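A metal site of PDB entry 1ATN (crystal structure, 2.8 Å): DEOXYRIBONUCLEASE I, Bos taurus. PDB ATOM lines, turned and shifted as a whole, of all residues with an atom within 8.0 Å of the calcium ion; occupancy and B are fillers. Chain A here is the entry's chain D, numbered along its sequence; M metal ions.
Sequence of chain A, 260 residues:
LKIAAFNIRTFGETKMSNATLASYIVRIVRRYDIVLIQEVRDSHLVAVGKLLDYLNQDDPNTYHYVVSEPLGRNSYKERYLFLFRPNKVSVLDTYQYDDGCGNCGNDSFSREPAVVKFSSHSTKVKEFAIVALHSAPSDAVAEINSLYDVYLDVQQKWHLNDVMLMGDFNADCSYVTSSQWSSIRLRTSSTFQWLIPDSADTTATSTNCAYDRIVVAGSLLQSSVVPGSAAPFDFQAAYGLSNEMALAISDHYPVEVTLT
Five residues have an atom within 4 Å of the calcium ion: Asp 99, Cys 101, Asp 107, Phe 109 and Glu 112.
Along chain A the residues within 4 Å of the calcium ion span positions 99 to 112.
NH1 of Arg 73 is in salt-bridge range of OD1 of Asp 107 (3.6 Å).
The backbone carbonyl oxygen of Asp 99 sits at hydrogen-bond distance from the backbone NH of Ser 108 (3.0 Å).
The side-chain sulfur (SG) of Cys 101 forms a disulfide with the side-chain sulfur (SG) of Cys 104.
The calcium ion is bound by OE2 of Glu 112 (2.5 Å), OD2 of Asp 107 (2.5 Å), OD2 of Asp 99 (2.5 Å), O of Cys 101 (2.5 Å) and O of Phe 109 (2.6 Å).
The calcium ion has five donor atoms within binding distance.
Slightly farther from the calcium ion lies OD1 of Asp 99 (3.0 Å).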
ATOM      1  N   LEU A  71     -24.428  12.356 -29.335  1.00  0.00           N
ATOM      2  CA  LEU A  71     -23.257  12.847 -28.657  1.00  0.00           C
ATOM      3  C   LEU A  71     -22.421  11.709 -28.068  1.00  0.00           C
ATOM      4  O   LEU A  71     -22.991  10.821 -27.423  1.00  0.00           O
ATOM      5  CB  LEU A  71     -23.754  13.801 -27.542  1.00  0.00           C
ATOM      6  CG  LEU A  71     -23.872  15.346 -27.626  1.00  0.00           C
ATOM      7  CD1 LEU A  71     -24.018  15.789 -29.047  1.00  0.00           C
ATOM      8  CD2 LEU A  71     -25.008  15.791 -26.730  1.00  0.00           C
ATOM      9  N   GLY A  72     -21.092  11.686 -28.215  1.00  0.00           N
ATOM     10  CA  GLY A  72     -20.288  10.677 -27.553  1.00  0.00           C
ATOM     11  C   GLY A  72     -18.923  10.458 -28.197  1.00  0.00           C
ATOM     12  O   GLY A  72     -18.893  10.139 -29.379  1.00  0.00           O
ATOM     13  N   ARG A  73     -17.773  10.645 -27.507  1.00  0.00           N
ATOM     14  CA  ARG A  73     -16.451  10.268 -28.076  1.00  0.00           C
ATOM     15  C   ARG A  73     -16.389   8.731 -28.215  1.00  0.00           C
ATOM     16  O   ARG A  73     -16.052   8.128 -29.251  1.00  0.00           O
ATOM     17  CB  ARG A  73     -15.245  10.777 -27.194  1.00  0.00           C
ATOM     18  CG  ARG A  73     -15.263  10.801 -25.661  1.00  0.00           C
ATOM     19  CD  ARG A  73     -14.231  11.766 -25.016  1.00  0.00           C
ATOM     20  NE  ARG A  73     -14.356  11.849 -23.551  1.00  0.00           N
ATOM     21  CZ  ARG A  73     -14.228  13.012 -22.839  1.00  0.00           C
ATOM     22  NH1 ARG A  73     -13.911  14.178 -23.436  1.00  0.00           N
ATOM     23  NH2 ARG A  73     -14.415  13.036 -21.512  1.00  0.00           N
ATOM     24  N   ASN A  74     -16.931   8.186 -27.109  1.00  0.00           N
ATOM     25  CA  ASN A  74     -17.207   6.770 -26.922  1.00  0.00           C
ATOM     26  C   ASN A  74     -17.671   6.057 -28.173  1.00  0.00           C
ATOM     27  O   ASN A  74     -17.167   5.006 -28.513  1.00  0.00           O
ATOM     28  CB  ASN A  74     -18.288   6.616 -25.795  1.00  0.00           C
ATOM     29  CG  ASN A  74     -19.342   7.744 -25.617  1.00  0.00           C
ATOM     30  OD1 ASN A  74     -19.000   8.824 -25.113  1.00  0.00           O
ATOM     31  ND2 ASN A  74     -20.621   7.565 -25.973  1.00  0.00           N
ATOM     32  N   TYR A  97     -22.388  23.482 -26.866  1.00  0.00           N
ATOM     33  CA  TYR A  97     -21.095  23.875 -26.408  1.00  0.00           C
ATOM     34  C   TYR A  97     -20.037  23.248 -27.270  1.00  0.00           C
ATOM     35  O   TYR A  97     -20.109  22.097 -27.723  1.00  0.00           O
ATOM     36  CB  TYR A  97     -20.885  23.431 -25.006  1.00  0.00           C
ATOM     37  CG  TYR A  97     -19.522  23.837 -24.458  1.00  0.00           C
ATOM     38  CD1 TYR A  97     -19.271  25.182 -24.271  1.00  0.00           C
ATOM     39  CD2 TYR A  97     -18.544  22.895 -24.219  1.00  0.00           C
ATOM     40  CE1 TYR A  97     -18.027  25.589 -23.846  1.00  0.00           C
ATOM     41  CE2 TYR A  97     -17.285  23.296 -23.799  1.00  0.00           C
ATOM     42  CZ  TYR A  97     -17.049  24.642 -23.624  1.00  0.00           C
ATOM     43  OH  TYR A  97     -15.791  25.087 -23.264  1.00  0.00           O
ATOM     44  N   ASP A  98     -19.058  24.083 -27.547  1.00  0.00           N
ATOM     45  CA  ASP A  98     -17.956  23.601 -28.336  1.00  0.00           C
ATOM     46  C   ASP A  98     -16.798  23.054 -27.514  1.00  0.00           C
ATOM     47  O   ASP A  98     -15.860  23.803 -27.215  1.00  0.00           O
ATOM     48  CB  ASP A  98     -17.474  24.724 -29.188  1.00  0.00           C
ATOM     49  CG  ASP A  98     -16.641  24.226 -30.369  1.00  0.00           C
ATOM     50  OD1 ASP A  98     -16.326  23.018 -30.459  1.00  0.00           O
ATOM     51  OD2 ASP A  98     -16.327  25.075 -31.227  1.00  0.00           O
ATOM     52  N   ASP A  99     -16.819  21.757 -27.155  1.00  0.00           N
ATOM     53  CA  ASP A  99     -15.811  21.187 -26.270  1.00  0.00           C
ATOM     54  C   ASP A  99     -14.449  20.770 -26.913  1.00  0.00           C
ATOM     55  O   ASP A  99     -13.637  20.115 -26.260  1.00  0.00           O
ATOM     56  CB  ASP A  99     -16.498  19.995 -25.551  1.00  0.00           C
ATOM     57  CG  ASP A  99     -16.467  18.675 -26.306  1.00  0.00           C
ATOM     58  OD1 ASP A  99     -16.652  18.666 -27.505  1.00  0.00           O
ATOM     59  OD2 ASP A  99     -16.250  17.612 -25.740  1.00  0.00           O
ATOM     60  N   GLY A 100     -14.156  21.115 -28.176  1.00  0.00           N
ATOM     61  CA  GLY A 100     -12.890  20.742 -28.788  1.00  0.00           C
ATOM     62  C   GLY A 100     -12.924  19.471 -29.652  1.00  0.00           C
ATOM     63  O   GLY A 100     -11.868  18.952 -30.052  1.00  0.00           O
ATOM     64  N   CYS A 101     -14.176  19.009 -29.905  1.00  0.00           N
ATOM     65  CA  CYS A 101     -14.610  17.866 -30.726  1.00  0.00           C
ATOM     66  C   CYS A 101     -16.059  17.643 -30.197  1.00  0.00           C
ATOM     67  O   CYS A 101     -16.289  16.633 -29.500  1.00  0.00           O
ATOM     68  CB  CYS A 101     -13.791  16.516 -30.533  1.00  0.00           C
ATOM     69  SG  CYS A 101     -12.301  15.915 -31.397  1.00  0.00           S
ATOM     70  N   CYS A 104      -9.337  13.871 -32.262  1.00  0.00           N
ATOM     71  CA  CYS A 104      -8.430  14.939 -31.842  1.00  0.00           C
ATOM     72  C   CYS A 104      -7.638  14.610 -30.565  1.00  0.00           C
ATOM     73  O   CYS A 104      -6.410  14.736 -30.530  1.00  0.00           O
ATOM     74  CB  CYS A 104      -9.218  16.304 -31.626  1.00  0.00           C
ATOM     75  SG  CYS A 104     -10.586  16.494 -30.416  1.00  0.00           S
ATOM     76  N   ASN A 106      -8.501  16.199 -27.360  1.00  0.00           N
ATOM     77  CA  ASN A 106      -8.653  17.218 -26.310  1.00  0.00           C
ATOM     78  C   ASN A 106     -10.036  17.349 -25.701  1.00  0.00           C
ATOM     79  O   ASN A 106     -10.121  17.628 -24.501  1.00  0.00           O
ATOM     80  CB  ASN A 106      -8.255  18.661 -26.788  1.00  0.00           C
ATOM     81  CG  ASN A 106      -9.360  19.633 -27.321  1.00  0.00           C
ATOM     82  OD1 ASN A 106     -10.031  20.365 -26.578  1.00  0.00           O
ATOM     83  ND2 ASN A 106      -9.561  19.678 -28.642  1.00  0.00           N
ATOM     84  N   ASP A 107     -11.081  17.138 -26.500  1.00  0.00           N
ATOM     85  CA  ASP A 107     -12.427  17.461 -26.119  1.00  0.00           C
ATOM     86  C   ASP A 107     -12.772  17.181 -24.682  1.00  0.00           C
ATOM     87  O   ASP A 107     -12.462  16.132 -24.103  1.00  0.00           O
ATOM     88  CB  ASP A 107     -13.306  16.723 -27.075  1.00  0.00           C
ATOM     89  CG  ASP A 107     -13.434  15.260 -26.739  1.00  0.00           C
ATOM     90  OD1 ASP A 107     -12.430  14.565 -26.707  1.00  0.00           O
ATOM     91  OD2 ASP A 107     -14.555  14.832 -26.465  1.00  0.00           O
ATOM     92  N   SER A 108     -13.253  18.215 -24.026  1.00  0.00           N
ATOM     93  CA  SER A 108     -13.489  18.113 -22.598  1.00  0.00           C
ATOM     94  C   SER A 108     -14.664  17.292 -22.178  1.00  0.00           C
ATOM     95  O   SER A 108     -14.639  16.892 -21.025  1.00  0.00           O
ATOM     96  CB  SER A 108     -13.643  19.496 -21.990  1.00  0.00           C
ATOM     97  OG  SER A 108     -14.154  20.487 -22.873  1.00  0.00           O
ATOM     98  N   PHE A 109     -15.654  16.995 -23.008  1.00  0.00           N
ATOM     99  CA  PHE A 109     -16.791  16.161 -22.621  1.00  0.00           C
ATOM    100  C   PHE A 109     -17.172  15.030 -23.560  1.00  0.00           C
ATOM    101  O   PHE A 109     -17.024  15.056 -24.780  1.00  0.00           O
ATOM    102  CB  PHE A 109     -18.090  16.936 -22.455  1.00  0.00           C
ATOM    103  CG  PHE A 109     -18.016  18.119 -21.538  1.00  0.00           C
ATOM    104  CD1 PHE A 109     -17.585  19.334 -22.031  1.00  0.00           C
ATOM    105  CD2 PHE A 109     -18.436  18.014 -20.232  1.00  0.00           C
ATOM    106  CE1 PHE A 109     -17.573  20.441 -21.206  1.00  0.00           C
ATOM    107  CE2 PHE A 109     -18.415  19.137 -19.417  1.00  0.00           C
ATOM    108  CZ  PHE A 109     -17.988  20.340 -19.907  1.00  0.00           C
ATOM    109  N   SER A 110     -17.744  14.035 -22.892  1.00  0.00           N
ATOM    110  CA  SER A 110     -18.278  12.853 -23.550  1.00  0.00           C
ATOM    111  C   SER A 110     -19.430  13.332 -24.419  1.00  0.00           C
ATOM    112  O   SER A 110     -19.388  13.128 -25.640  1.00  0.00           O
ATOM    113  CB  SER A 110     -18.746  11.843 -22.472  1.00  0.00           C
ATOM    114  OG  SER A 110     -19.257  10.606 -23.002  1.00  0.00           O
ATOM    115  N   ARG A 111     -20.375  14.046 -23.781  1.00  0.00           N
ATOM    116  CA  ARG A 111     -21.603  14.611 -24.343  1.00  0.00           C
ATOM    117  C   ARG A 111     -21.725  16.096 -24.016  1.00  0.00           C
ATOM    118  O   ARG A 111     -22.317  16.479 -22.998  1.00  0.00           O
ATOM    119  CB  ARG A 111     -22.758  13.910 -23.771  1.00  0.00           C
ATOM    120  CG  ARG A 111     -22.705  12.497 -24.183  1.00  0.00           C
ATOM    121  CD  ARG A 111     -23.576  11.754 -23.227  1.00  0.00           C
ATOM    122  NE  ARG A 111     -23.010  11.557 -21.905  1.00  0.00           N
ATOM    123  CZ  ARG A 111     -22.676  10.330 -21.475  1.00  0.00           C
ATOM    124  NH1 ARG A 111     -22.649   9.274 -22.297  1.00  0.00           N
ATOM    125  NH2 ARG A 111     -22.364  10.172 -20.196  1.00  0.00           N
ATOM    126  N   GLU A 112     -21.104  16.889 -24.868  1.00  0.00           N
ATOM    127  CA  GLU A 112     -21.092  18.342 -24.870  1.00  0.00           C
ATOM    128  C   GLU A 112     -22.435  18.930 -24.466  1.00  0.00           C
ATOM    129  O   GLU A 112     -23.432  18.653 -25.152  1.00  0.00           O
ATOM    130  CB  GLU A 112     -20.866  18.966 -26.214  1.00  0.00           C
ATOM    131  CG  GLU A 112     -19.734  18.638 -27.076  1.00  0.00           C
ATOM    132  CD  GLU A 112     -19.709  17.208 -27.604  1.00  0.00           C
ATOM    133  OE1 GLU A 112     -20.290  16.933 -28.638  1.00  0.00           O
ATOM    134  OE2 GLU A 112     -19.065  16.365 -26.979  1.00  0.00           O
ATOM    135  N   GLU A 143     -15.260  16.899 -15.846  1.00  0.00           N
ATOM    136  CA  GLU A 143     -16.417  17.470 -16.501  1.00  0.00           C
ATOM    137  C   GLU A 143     -17.250  18.420 -15.588  1.00  0.00           C
ATOM    138  O   GLU A 143     -17.548  19.527 -16.028  1.00  0.00           O
ATOM    139  CB  GLU A 143     -17.220  16.294 -17.037  1.00  0.00           C
ATOM    140  CG  GLU A 143     -16.452  15.645 -18.116  1.00  0.00           C
ATOM    141  CD  GLU A 143     -17.205  14.686 -18.994  1.00  0.00           C
ATOM    142  OE1 GLU A 143     -18.292  14.219 -18.686  1.00  0.00           O
ATOM    143  OE2 GLU A 143     -16.662  14.379 -20.038  1.00  0.00           O
HETATM  144 CA    CA M   1     -16.715  15.711 -27.225  1.00  0.00          CA
